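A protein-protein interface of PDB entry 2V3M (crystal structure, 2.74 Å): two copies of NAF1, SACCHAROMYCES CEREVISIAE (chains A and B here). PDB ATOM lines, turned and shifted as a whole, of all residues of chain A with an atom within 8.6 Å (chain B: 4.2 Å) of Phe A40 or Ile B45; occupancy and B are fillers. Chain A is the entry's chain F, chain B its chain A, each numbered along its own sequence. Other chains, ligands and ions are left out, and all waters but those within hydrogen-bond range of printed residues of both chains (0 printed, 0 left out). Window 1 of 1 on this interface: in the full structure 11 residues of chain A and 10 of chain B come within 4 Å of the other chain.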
ATOM      1  N   LEU A  36     -13.401 -19.694  -1.037  1.00  0.00           N
ATOM      2  CA  LEU A  36     -14.545 -19.141  -0.365  1.00  0.00           C
ATOM      3  C   LEU A  36     -14.951 -17.953  -1.212  1.00  0.00           C
ATOM      4  O   LEU A  36     -14.165 -17.033  -1.406  1.00  0.00           O
ATOM      5  CB  LEU A  36     -14.133 -18.756   1.056  1.00  0.00           C
ATOM      6  CG  LEU A  36     -14.912 -17.841   1.966  1.00  0.00           C
ATOM      7  CD1 LEU A  36     -16.229 -18.388   2.198  1.00  0.00           C
ATOM      8  CD2 LEU A  36     -14.194 -17.751   3.253  1.00  0.00           C
ATOM      9  N   LYS A  37     -16.152 -17.965  -1.775  1.00  0.00           N
ATOM     10  CA  LYS A  37     -16.529 -16.847  -2.642  1.00  0.00           C
ATOM     11  C   LYS A  37     -17.592 -15.872  -2.087  1.00  0.00           C
ATOM     12  O   LYS A  37     -17.693 -14.780  -2.557  1.00  0.00           O
ATOM     13  CB  LYS A  37     -16.996 -17.352  -4.014  1.00  0.00           C
ATOM     14  CG  LYS A  37     -15.915 -17.812  -4.904  1.00  0.00           C
ATOM     15  CD  LYS A  37     -15.120 -16.682  -5.442  1.00  0.00           C
ATOM     16  CE  LYS A  37     -14.041 -17.169  -6.360  1.00  0.00           C
ATOM     17  NZ  LYS A  37     -13.243 -16.015  -6.806  1.00  0.00           N
ATOM     18  N   SER A  38     -18.415 -16.272  -1.132  1.00  0.00           N
ATOM     19  CA  SER A  38     -19.498 -15.367  -0.764  1.00  0.00           C
ATOM     20  C   SER A  38     -20.082 -15.624   0.640  1.00  0.00           C
ATOM     21  O   SER A  38     -20.136 -16.783   1.143  1.00  0.00           O
ATOM     22  CB  SER A  38     -20.579 -15.504  -1.843  1.00  0.00           C
ATOM     23  OG  SER A  38     -21.481 -14.471  -1.734  1.00  0.00           O
ATOM     24  N   ALA A  39     -20.516 -14.563   1.295  1.00  0.00           N
ATOM     25  CA  ALA A  39     -21.187 -14.767   2.561  1.00  0.00           C
ATOM     26  C   ALA A  39     -22.337 -13.830   2.591  1.00  0.00           C
ATOM     27  O   ALA A  39     -22.120 -12.643   2.482  1.00  0.00           O
ATOM     28  CB  ALA A  39     -20.239 -14.478   3.662  1.00  0.00           C
ATOM     29  N   PHE A  40     -23.544 -14.360   2.714  1.00  0.00           N
ATOM     30  CA  PHE A  40     -24.780 -13.555   2.922  1.00  0.00           C
ATOM     31  C   PHE A  40     -25.816 -14.385   3.705  1.00  0.00           C
ATOM     32  O   PHE A  40     -25.888 -15.661   3.543  1.00  0.00           O
ATOM     33  CB  PHE A  40     -25.353 -13.138   1.591  1.00  0.00           C
ATOM     34  CG  PHE A  40     -25.745 -14.323   0.714  1.00  0.00           C
ATOM     35  CD1 PHE A  40     -27.061 -14.836   0.756  1.00  0.00           C
ATOM     36  CD2 PHE A  40     -24.796 -14.950  -0.108  1.00  0.00           C
ATOM     37  CE1 PHE A  40     -27.432 -15.878  -0.038  1.00  0.00           C
ATOM     38  CE2 PHE A  40     -25.143 -16.000  -0.883  1.00  0.00           C
ATOM     39  CZ  PHE A  40     -26.453 -16.506  -0.838  1.00  0.00           C
ATOM     40  N   GLU A  41     -26.578 -13.724   4.556  1.00  0.00           N
ATOM     41  CA  GLU A  41     -27.612 -14.363   5.298  1.00  0.00           C
ATOM     42  C   GLU A  41     -27.208 -15.665   5.951  1.00  0.00           C
ATOM     43  O   GLU A  41     -27.862 -16.700   5.785  1.00  0.00           O
ATOM     44  CB  GLU A  41     -28.786 -14.565   4.408  1.00  0.00           C
ATOM     45  CG  GLU A  41     -29.745 -13.392   4.615  1.00  0.00           C
ATOM     46  CD  GLU A  41     -30.973 -13.517   3.788  1.00  0.00           C
ATOM     47  OE1 GLU A  41     -32.043 -13.168   4.288  1.00  0.00           O
ATOM     48  OE2 GLU A  41     -30.820 -13.999   2.649  1.00  0.00           O
ATOM     49  N   ASN A  42     -26.122 -15.605   6.699  1.00  0.00           N
ATOM     50  CA  ASN A  42     -25.606 -16.777   7.353  1.00  0.00           C
ATOM     51  C   ASN A  42     -25.245 -17.934   6.419  1.00  0.00           C
ATOM     52  O   ASN A  42     -24.955 -19.052   6.888  1.00  0.00           O
ATOM     53  CB  ASN A  42     -26.578 -17.292   8.400  1.00  0.00           C
ATOM     54  CG  ASN A  42     -26.607 -16.428   9.629  1.00  0.00           C
ATOM     55  OD1 ASN A  42     -25.555 -16.014  10.129  1.00  0.00           O
ATOM     56  ND2 ASN A  42     -27.801 -16.116  10.116  1.00  0.00           N
ATOM     57  N   ASN A  43     -25.218 -17.699   5.117  1.00  0.00           N
ATOM     58  CA  ASN A  43     -24.747 -18.785   4.279  1.00  0.00           C
ATOM     59  C   ASN A  43     -23.343 -18.459   3.873  1.00  0.00           C
ATOM     60  O   ASN A  43     -23.009 -17.238   3.636  1.00  0.00           O
ATOM     61  CB  ASN A  43     -25.607 -18.918   3.037  1.00  0.00           C
ATOM     62  CG  ASN A  43     -26.979 -19.401   3.352  1.00  0.00           C
ATOM     63  OD1 ASN A  43     -27.226 -20.609   3.409  1.00  0.00           O
ATOM     64  ND2 ASN A  43     -27.890 -18.455   3.611  1.00  0.00           N
ATOM     65  N   ILE A  44     -22.518 -19.494   3.764  1.00  0.00           N
ATOM     66  CA  ILE A  44     -21.206 -19.342   3.161  1.00  0.00           C
ATOM     67  C   ILE A  44     -21.126 -20.121   1.848  1.00  0.00           C
ATOM     68  O   ILE A  44     -21.549 -21.303   1.794  1.00  0.00           O
ATOM     69  CB  ILE A  44     -20.104 -19.873   4.118  1.00  0.00           C
ATOM     70  CG1 ILE A  44     -20.086 -19.077   5.407  1.00  0.00           C
ATOM     71  CG2 ILE A  44     -18.718 -19.812   3.498  1.00  0.00           C
ATOM     72  CD1 ILE A  44     -20.241 -17.590   5.192  1.00  0.00           C
ATOM     73  N   ILE A  45     -20.634 -19.499   0.770  1.00  0.00           N
ATOM     74  CA  ILE A  45     -20.659 -20.188  -0.527  1.00  0.00           C
ATOM     75  C   ILE A  45     -19.244 -20.491  -0.940  1.00  0.00           C
ATOM     76  O   ILE A  45     -18.437 -19.598  -0.998  1.00  0.00           O
ATOM     77  CB  ILE A  45     -21.241 -19.327  -1.622  1.00  0.00           C
ATOM     78  CG1 ILE A  45     -22.761 -19.224  -1.558  1.00  0.00           C
ATOM     79  CG2 ILE A  45     -20.959 -19.984  -3.018  1.00  0.00           C
ATOM     80  CD1 ILE A  45     -23.471 -19.856  -0.521  1.00  0.00           C
ATOM     81  N   ILE A  46     -18.960 -21.716  -1.306  1.00  0.00           N
ATOM     82  CA  ILE A  46     -17.668 -22.098  -1.773  1.00  0.00           C
ATOM     83  C   ILE A  46     -17.604 -22.502  -3.222  1.00  0.00           C
ATOM     84  O   ILE A  46     -18.472 -23.232  -3.652  1.00  0.00           O
ATOM     85  CB  ILE A  46     -17.186 -23.203  -0.859  1.00  0.00           C
ATOM     86  CG1 ILE A  46     -17.102 -22.482   0.535  1.00  0.00           C
ATOM     87  CG2 ILE A  46     -15.858 -23.785  -1.401  1.00  0.00           C
ATOM     88  CD1 ILE A  46     -16.484 -22.999   1.676  1.00  0.00           C
ATOM     89  N   PHE A  78     -24.984 -27.052  -5.257  1.00  0.00           N
ATOM     90  CA  PHE A  78     -25.649 -26.606  -6.470  1.00  0.00           C
ATOM     91  C   PHE A  78     -24.658 -26.163  -7.595  1.00  0.00           C
ATOM     92  O   PHE A  78     -23.466 -26.302  -7.492  1.00  0.00           O
ATOM     93  CB  PHE A  78     -26.586 -25.460  -6.094  1.00  0.00           C
ATOM     94  CG  PHE A  78     -25.890 -24.255  -5.602  1.00  0.00           C
ATOM     95  CD1 PHE A  78     -25.372 -24.203  -4.374  1.00  0.00           C
ATOM     96  CD2 PHE A  78     -25.772 -23.134  -6.375  1.00  0.00           C
ATOM     97  CE1 PHE A  78     -24.699 -22.993  -3.906  1.00  0.00           C
ATOM     98  CE2 PHE A  78     -25.049 -21.914  -5.904  1.00  0.00           C
ATOM     99  CZ  PHE A  78     -24.517 -21.875  -4.722  1.00  0.00           C
ATOM    100  N   PHE A  85     -20.965 -25.429  -6.687  1.00  0.00           N
ATOM    101  CA  PHE A  85     -20.802 -24.535  -5.645  1.00  0.00           C
ATOM    102  C   PHE A  85     -21.228 -25.237  -4.429  1.00  0.00           C
ATOM    103  O   PHE A  85     -22.177 -25.996  -4.500  1.00  0.00           O
ATOM    104  CB  PHE A  85     -21.757 -23.372  -5.777  1.00  0.00           C
ATOM    105  CG  PHE A  85     -21.428 -22.430  -6.884  1.00  0.00           C
ATOM    106  CD1 PHE A  85     -22.147 -22.472  -8.119  1.00  0.00           C
ATOM    107  CD2 PHE A  85     -20.420 -21.539  -6.738  1.00  0.00           C
ATOM    108  CE1 PHE A  85     -21.835 -21.652  -9.164  1.00  0.00           C
ATOM    109  CE2 PHE A  85     -20.092 -20.662  -7.772  1.00  0.00           C
ATOM    110  CZ  PHE A  85     -20.777 -20.709  -8.969  1.00  0.00           C
ATOM    111  N   TYR A  86     -20.642 -24.917  -3.275  1.00  0.00           N
ATOM    112  CA  TYR A  86     -21.113 -25.479  -2.010  1.00  0.00           C
ATOM    113  C   TYR A  86     -21.701 -24.411  -1.090  1.00  0.00           C
ATOM    114  O   TYR A  86     -21.134 -23.331  -0.930  1.00  0.00           O
ATOM    115  CB  TYR A  86     -19.990 -26.217  -1.278  1.00  0.00           C
ATOM    116  CG  TYR A  86     -19.306 -27.199  -2.181  1.00  0.00           C
ATOM    117  CD1 TYR A  86     -17.961 -27.073  -2.503  1.00  0.00           C
ATOM    118  CD2 TYR A  86     -20.041 -28.220  -2.779  1.00  0.00           C
ATOM    119  CE1 TYR A  86     -17.338 -27.951  -3.352  1.00  0.00           C
ATOM    120  CE2 TYR A  86     -19.415 -29.138  -3.604  1.00  0.00           C
ATOM    121  CZ  TYR A  86     -18.067 -28.991  -3.902  1.00  0.00           C
ATOM    122  OH  TYR A  86     -17.440 -29.897  -4.709  1.00  0.00           O
ATOM    123  N   ARG A  87     -22.841 -24.714  -0.483  1.00  0.00           N
ATOM    124  CA  ARG A  87     -23.448 -23.814   0.404  1.00  0.00           C
ATOM    125  C   ARG A  87     -23.382 -24.431   1.777  1.00  0.00           C
ATOM    126  O   ARG A  87     -23.784 -25.627   1.937  1.00  0.00           O
ATOM    127  CB  ARG A  87     -24.882 -23.716  -0.012  1.00  0.00           C
ATOM    128  CG  ARG A  87     -25.662 -22.671   0.757  1.00  0.00           C
ATOM    129  CD  ARG A  87     -27.088 -22.676   0.224  1.00  0.00           C
ATOM    130  NE  ARG A  87     -27.936 -22.599   1.373  1.00  0.00           N
ATOM    131  CZ  ARG A  87     -28.813 -23.477   1.686  1.00  0.00           C
ATOM    132  NH1 ARG A  87     -29.087 -24.448   0.892  1.00  0.00           N
ATOM    133  NH2 ARG A  87     -29.435 -23.302   2.808  1.00  0.00           N
ATOM    134  N   ILE A  88     -22.878 -23.647   2.745  1.00  0.00           N
ATOM    135  CA  ILE A  88     -22.843 -24.016   4.172  1.00  0.00           C
ATOM    136  C   ILE A  88     -23.693 -23.000   4.921  1.00  0.00           C
ATOM    137  O   ILE A  88     -23.355 -21.788   4.950  1.00  0.00           O
ATOM    138  CB  ILE A  88     -21.392 -23.992   4.790  1.00  0.00           C
ATOM    139  CG1 ILE A  88     -20.507 -25.069   4.121  1.00  0.00           C
ATOM    140  CG2 ILE A  88     -21.388 -24.373   6.297  1.00  0.00           C
ATOM    141  CD1 ILE A  88     -19.516 -24.615   3.014  1.00  0.00           C
ATOM    142  N   LYS A  89     -24.776 -23.474   5.532  1.00  0.00           N
ATOM    143  CA  LYS A  89     -25.610 -22.594   6.297  1.00  0.00           C
ATOM    144  C   LYS A  89     -25.133 -22.627   7.713  1.00  0.00           C
ATOM    145  O   LYS A  89     -25.103 -23.699   8.283  1.00  0.00           O
ATOM    146  CB  LYS A  89     -27.044 -23.097   6.236  1.00  0.00           C
ATOM    147  CG  LYS A  89     -27.984 -22.417   7.117  1.00  0.00           C
ATOM    148  CD  LYS A  89     -28.295 -20.975   6.653  1.00  0.00           C
ATOM    149  CE  LYS A  89     -29.543 -20.515   7.403  1.00  0.00           C
ATOM    150  NZ  LYS A  89     -29.947 -19.111   7.049  1.00  0.00           N
ATOM    151  N   LEU A  90     -24.744 -21.483   8.289  1.00  0.00           N
ATOM    152  CA  LEU A  90     -24.418 -21.444   9.702  1.00  0.00           C
ATOM    153  C   LEU A  90     -25.614 -21.069  10.505  1.00  0.00           C
ATOM    154  O   LEU A  90     -26.416 -20.300  10.037  1.00  0.00           O
ATOM    155  CB  LEU A  90     -23.394 -20.345   9.948  1.00  0.00           C
ATOM    156  CG  LEU A  90     -22.114 -20.388   9.154  1.00  0.00           C
ATOM    157  CD1 LEU A  90     -21.404 -19.261   9.615  1.00  0.00           C
ATOM    158  CD2 LEU A  90     -21.293 -21.569   9.466  1.00  0.00           C
ATOM    159  N   PHE A  98     -19.635 -16.153  11.091  1.00  0.00           N
ATOM    160  CA  PHE A  98     -20.028 -15.596   9.805  1.00  0.00           C
ATOM    161  C   PHE A  98     -19.218 -14.301   9.581  1.00  0.00           C
ATOM    162  O   PHE A  98     -18.501 -14.148   8.598  1.00  0.00           O
ATOM    163  CB  PHE A  98     -21.511 -15.344   9.792  1.00  0.00           C
ATOM    164  CG  PHE A  98     -22.003 -14.725   8.559  1.00  0.00           C
ATOM    165  CD1 PHE A  98     -22.266 -15.498   7.458  1.00  0.00           C
ATOM    166  CD2 PHE A  98     -22.237 -13.350   8.504  1.00  0.00           C
ATOM    167  CE1 PHE A  98     -22.755 -14.930   6.273  1.00  0.00           C
ATOM    168  CE2 PHE A  98     -22.733 -12.718   7.337  1.00  0.00           C
ATOM    169  CZ  PHE A  98     -22.988 -13.530   6.186  1.00  0.00           C
ATOM    170  N   LEU A 101     -15.848 -14.850   8.517  1.00  0.00           N
ATOM    171  CA  LEU A 101     -15.647 -15.473   7.235  1.00  0.00           C
ATOM    172  C   LEU A 101     -16.007 -14.480   6.154  1.00  0.00           C
ATOM    173  O   LEU A 101     -15.322 -14.419   5.124  1.00  0.00           O
ATOM    174  CB  LEU A 101     -16.457 -16.778   7.088  1.00  0.00           C
ATOM    175  CG  LEU A 101     -16.194 -17.844   8.176  1.00  0.00           C
ATOM    176  CD1 LEU A 101     -16.981 -19.032   7.957  1.00  0.00           C
ATOM    177  CD2 LEU A 101     -14.844 -18.302   8.030  1.00  0.00           C
ATOM    178  N   LYS A 102     -17.051 -13.687   6.408  1.00  0.00           N
ATOM    179  CA  LYS A 102     -17.462 -12.562   5.544  1.00  0.00           C
ATOM    180  C   LYS A 102     -16.243 -11.790   5.089  1.00  0.00           C
ATOM    181  O   LYS A 102     -16.152 -11.294   4.028  1.00  0.00           O
ATOM    182  CB  LYS A 102     -18.351 -11.642   6.384  1.00  0.00           C
ATOM    183  CG  LYS A 102     -18.859 -10.389   5.752  1.00  0.00           C
ATOM    184  CD  LYS A 102     -20.147 -10.715   4.996  1.00  0.00           C
ATOM    185  CE  LYS A 102     -20.764  -9.519   4.229  1.00  0.00           C
ATOM    186  NZ  LYS A 102     -22.256  -9.700   4.018  1.00  0.00           N
ATOM    187  N   LEU A 105     -13.156 -13.619   2.253  1.00  0.00           N
ATOM    188  CA  LEU A 105     -13.517 -14.071   0.919  1.00  0.00           C
ATOM    189  C   LEU A 105     -12.288 -14.206   0.077  1.00  0.00           C
ATOM    190  O   LEU A 105     -11.378 -13.372   0.139  1.00  0.00           O
ATOM    191  CB  LEU A 105     -14.427 -13.059   0.249  1.00  0.00           C
ATOM    192  CG  LEU A 105     -15.911 -13.266   0.447  1.00  0.00           C
ATOM    193  CD1 LEU A 105     -16.311 -14.173   1.617  1.00  0.00           C
ATOM    194  CD2 LEU A 105     -16.559 -11.879   0.525  1.00  0.00           C
ATOM    195  N   LEU B  36     -31.776  -8.301  -3.340  1.00  0.00           N
ATOM    196  CA  LEU B  36     -30.473  -8.603  -3.926  1.00  0.00           C
ATOM    197  C   LEU B  36     -29.518  -8.860  -2.781  1.00  0.00           C
ATOM    198  O   LEU B  36     -29.319  -7.929  -1.940  1.00  0.00           O
ATOM    199  CB  LEU B  36     -30.062  -7.370  -4.720  1.00  0.00           C
ATOM    200  CG  LEU B  36     -28.697  -7.253  -5.402  1.00  0.00           C
ATOM    201  CD1 LEU B  36     -28.554  -8.271  -6.436  1.00  0.00           C
ATOM    202  CD2 LEU B  36     -28.543  -5.886  -6.082  1.00  0.00           C
ATOM    203  N   LYS B  37     -29.000 -10.088  -2.666  1.00  0.00           N
ATOM    204  CA  LYS B  37     -28.161 -10.410  -1.515  1.00  0.00           C
ATOM    205  C   LYS B  37     -26.694 -10.650  -1.790  1.00  0.00           C
ATOM    206  O   LYS B  37     -25.909 -10.475  -0.916  1.00  0.00           O
ATOM    207  CB  LYS B  37     -28.728 -11.563  -0.795  1.00  0.00           C
ATOM    208  CG  LYS B  37     -30.016 -11.171  -0.060  1.00  0.00           C
ATOM    209  CD  LYS B  37     -29.733 -10.351   1.144  1.00  0.00           C
ATOM    210  CE  LYS B  37     -30.890 -10.395   2.112  1.00  0.00           C
ATOM    211  NZ  LYS B  37     -30.592  -9.478   3.308  1.00  0.00           N
ATOM    212  N   SER B  38     -26.319 -10.967  -3.029  1.00  0.00           N
ATOM    213  CA  SER B  38     -24.959 -11.310  -3.302  1.00  0.00           C
ATOM    214  C   SER B  38     -24.468 -11.160  -4.769  1.00  0.00           C
ATOM    215  O   SER B  38     -25.232 -11.243  -5.713  1.00  0.00           O
ATOM    216  CB  SER B  38     -24.727 -12.728  -2.864  1.00  0.00           C
ATOM    217  OG  SER B  38     -23.347 -12.861  -2.694  1.00  0.00           O
ATOM    218  N   PHE B  40     -20.950 -12.394  -6.751  1.00  0.00           N
ATOM    219  CA  PHE B  40     -19.587 -12.926  -6.952  1.00  0.00           C
ATOM    220  C   PHE B  40     -19.509 -13.646  -8.293  1.00  0.00           C
ATOM    221  O   PHE B  40     -20.486 -14.268  -8.758  1.00  0.00           O
ATOM    222  CB  PHE B  40     -19.237 -13.851  -5.824  1.00  0.00           C
ATOM    223  CG  PHE B  40     -20.121 -15.032  -5.764  1.00  0.00           C
ATOM    224  CD1 PHE B  40     -19.749 -16.242  -6.378  1.00  0.00           C
ATOM    225  CD2 PHE B  40     -21.339 -14.949  -5.178  1.00  0.00           C
ATOM    226  CE1 PHE B  40     -20.617 -17.335  -6.390  1.00  0.00           C
ATOM    227  CE2 PHE B  40     -22.165 -16.020  -5.141  1.00  0.00           C
ATOM    228  CZ  PHE B  40     -21.787 -17.231  -5.762  1.00  0.00           C
ATOM    229  N   ASN B  43     -21.945 -13.914 -10.866  1.00  0.00           N
ATOM    230  CA  ASN B  43     -23.297 -14.294 -10.424  1.00  0.00           C
ATOM    231  C   ASN B  43     -23.963 -13.261  -9.524  1.00  0.00           C
ATOM    232  O   ASN B  43     -23.270 -12.656  -8.676  1.00  0.00           O
ATOM    233  CB  ASN B  43     -23.279 -15.582  -9.709  1.00  0.00           C
ATOM    234  CG  ASN B  43     -22.773 -16.695 -10.580  1.00  0.00           C
ATOM    235  OD1 ASN B  43     -23.568 -17.387 -11.285  1.00  0.00           O
ATOM    236  ND2 ASN B  43     -21.427 -16.944 -10.522  1.00  0.00           N
ATOM    237  N   ILE B  44     -25.268 -13.066  -9.704  1.00  0.00           N
ATOM    238  CA  ILE B  44     -26.030 -12.231  -8.830  1.00  0.00           C
ATOM    239  C   ILE B  44     -27.028 -13.171  -8.130  1.00  0.00           C
ATOM    240  O   ILE B  44     -27.700 -14.007  -8.760  1.00  0.00           O
ATOM    241  CB  ILE B  44     -26.790 -11.143  -9.636  1.00  0.00           C
ATOM    242  CG1 ILE B  44     -25.828 -10.180 -10.287  1.00  0.00           C
ATOM    243  CG2 ILE B  44     -27.772 -10.394  -8.776  1.00  0.00           C
ATOM    244  CD1 ILE B  44     -24.778  -9.754  -9.421  1.00  0.00           C
ATOM    245  N   ILE B  45     -27.104 -13.042  -6.820  1.00  0.00           N
ATOM    246  CA  ILE B  45     -27.931 -13.906  -6.026  1.00  0.00           C
ATOM    247  C   ILE B  45     -29.080 -13.092  -5.393  1.00  0.00           C
ATOM    248  O   ILE B  45     -28.818 -12.114  -4.716  1.00  0.00           O
ATOM    249  CB  ILE B  45     -27.146 -14.500  -4.898  1.00  0.00           C
ATOM    250  CG1 ILE B  45     -26.177 -15.482  -5.440  1.00  0.00           C
ATOM    251  CG2 ILE B  45     -28.044 -15.230  -3.987  1.00  0.00           C
ATOM    252  CD1 ILE B  45     -26.458 -16.079  -6.614  1.00  0.00           C
ATOM    253  N   ILE B  46     -30.308 -13.536  -5.578  1.00  0.00           N
ATOM    254  CA  ILE B  46     -31.481 -12.870  -5.001  1.00  0.00           C
ATOM    255  C   ILE B  46     -32.203 -13.794  -4.015  1.00  0.00           C
ATOM    256  O   ILE B  46     -32.386 -15.006  -4.312  1.00  0.00           O
ATOM    257  CB  ILE B  46     -32.455 -12.439  -6.159  1.00  0.00           C
ATOM    258  CG1 ILE B  46     -31.593 -11.559  -7.078  1.00  0.00           C
ATOM    259  CG2 ILE B  46     -33.792 -11.746  -5.619  1.00  0.00           C
ATOM    260  CD1 ILE B  46     -32.229 -10.771  -7.948  1.00  0.00           C
ATOM    261  N   PHE B  85     -33.475 -19.286  -3.416  1.00  0.00           N
ATOM    262  CA  PHE B  85     -32.515 -18.274  -3.845  1.00  0.00           C
ATOM    263  C   PHE B  85     -32.437 -18.357  -5.330  1.00  0.00           C
ATOM    264  O   PHE B  85     -32.441 -19.485  -5.858  1.00  0.00           O
ATOM    265  CB  PHE B  85     -31.111 -18.631  -3.441  1.00  0.00           C
ATOM    266  CG  PHE B  85     -30.840 -18.507  -1.979  1.00  0.00           C
ATOM    267  CD1 PHE B  85     -30.745 -19.636  -1.199  1.00  0.00           C
ATOM    268  CD2 PHE B  85     -30.646 -17.304  -1.399  1.00  0.00           C
ATOM    269  CE1 PHE B  85     -30.473 -19.556   0.186  1.00  0.00           C
ATOM    270  CE2 PHE B  85     -30.423 -17.184  -0.019  1.00  0.00           C
ATOM    271  CZ  PHE B  85     -30.319 -18.286   0.786  1.00  0.00           C
ATOM    272  N   TYR B  86     -32.354 -17.197  -5.993  1.00  0.00           N
ATOM    273  CA  TYR B  86     -32.327 -17.185  -7.410  1.00  0.00           C
ATOM    274  C   TYR B  86     -30.936 -16.807  -7.819  1.00  0.00           C
ATOM    275  O   TYR B  86     -30.329 -15.916  -7.236  1.00  0.00           O
ATOM    276  CB  TYR B  86     -33.312 -16.191  -7.876  1.00  0.00           C
ATOM    277  CG  TYR B  86     -34.687 -16.499  -7.434  1.00  0.00           C
ATOM    278  CD1 TYR B  86     -35.482 -15.532  -6.809  1.00  0.00           C
ATOM    279  CD2 TYR B  86     -35.218 -17.763  -7.605  1.00  0.00           C
ATOM    280  CE1 TYR B  86     -36.784 -15.819  -6.383  1.00  0.00           C
ATOM    281  CE2 TYR B  86     -36.516 -18.044  -7.256  1.00  0.00           C
ATOM    282  CZ  TYR B  86     -37.311 -17.074  -6.622  1.00  0.00           C
ATOM    283  OH  TYR B  86     -38.623 -17.410  -6.251  1.00  0.00           O
ATOM    284  N   ARG B  87     -30.377 -17.506  -8.785  1.00  0.00           N
ATOM    285  CA  ARG B  87     -29.066 -17.110  -9.290  1.00  0.00           C
ATOM    286  C   ARG B  87     -29.127 -16.654 -10.736  1.00  0.00           C
ATOM    287  O   ARG B  87     -29.665 -17.407 -11.625  1.00  0.00           O
ATOM    288  CB  ARG B  87     -28.176 -18.290  -9.138  1.00  0.00           C
ATOM    289  CG  ARG B  87     -26.722 -18.111  -9.491  1.00  0.00           C
ATOM    290  CD  ARG B  87     -26.134 -19.572  -9.545  1.00  0.00           C
ATOM    291  NE  ARG B  87     -25.346 -19.685 -10.730  1.00  0.00           N
ATOM    292  CZ  ARG B  87     -25.358 -20.672 -11.613  1.00  0.00           C
ATOM    293  NH1 ARG B  87     -26.099 -21.749 -11.483  1.00  0.00           N
ATOM    294  NH2 ARG B  87     -24.535 -20.603 -12.647  1.00  0.00           N
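Among the printed residues, pairs that only touch across the chains: Lys A37 with Phe B40, Ser A38 with Phe B40, Phe A40 with Lys B37, Phe A40 with Ser B38, Phe A40 with Ile B45, Phe A40 with Phe B85, Glu A41 with Lys B37, Asn A43 with Phe B85, Ile A45 with Phe B40 and Phe A85 with Phe B40.
OG of Ser B38 is in hydrogen-bond range of OG of Ser A38, 2.6 Å away.
The side-chain amide nitrogen of Asn B43 sits close to the backbone carbonyl oxygen of Phe B40 (3.3 Å). N of Lys A37 lies within hydrogen-bond range of O of Ile A45, at 2.9 Å. The backbone NH of Ile A45 is in hydrogen-bond range of the backbone carbonyl oxygen of Ser A38 (2.8 Å). ND2 of Asn A43 sits close to O of Phe A40. The side-chain amide nitrogen of Asn A43 lies within hydrogen-bond range of the backbone carbonyl oxygen of Glu A41. OD1 of Asn A43 lies within hydrogen-bond range of NE of Arg A87 (2.9 Å).
Of the 11 printed residues of chain B, 5 touch a printed residue of chain A. Among the printed residues, no Asp or Glu carboxylate lies within 4 Å of a Lys or Arg side-chain nitrogen of the other chain.
Phe A40 touches just these residues of chain B: Lys B37 (3.7 Å), Ser B38 (3.5 Å), Ile B45 (3.8 Å) and Phe B85 (3.3 Å). Ile B45 touches one residue of chain A. Of chain A, only Ser A38 and Phe A40 come within 4 Å of Ser B38. Of the printed residues of chain B, Phe A85 touches Phe B40 (3.6 Å). Of the printed residues of chain A, Phe B85 touches Phe A40 (3.3 Å) and Asn A43 (3.7 Å). Of the printed residues of chain A, Lys B37 touches Phe A40 and Glu A41. The nearest printed residue of chain B that does not touch Phe A40 is Phe B40 (5.2 Å). The nearest printed residue of chain B that does not touch Lys A37 is Ser B38 (6.0 Å).
Ser A38 touches its own counterpart, Ser B38. Ser A38 touches Phe B40, and with the chains exchanged Phe A40 touches Ser B38. Phe A40 touches Phe B85, and with the chains exchanged Phe A85 touches Phe B40. Asn A43 touches Phe B85, but with the chains exchanged Phe A85 does not touch Asn B43 (4.1 Å). 11 positions are printed for both chains. Of the 11 pairs that touch across the chains among the printed residues, 9 have their exchanged pair printed and touching as well.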
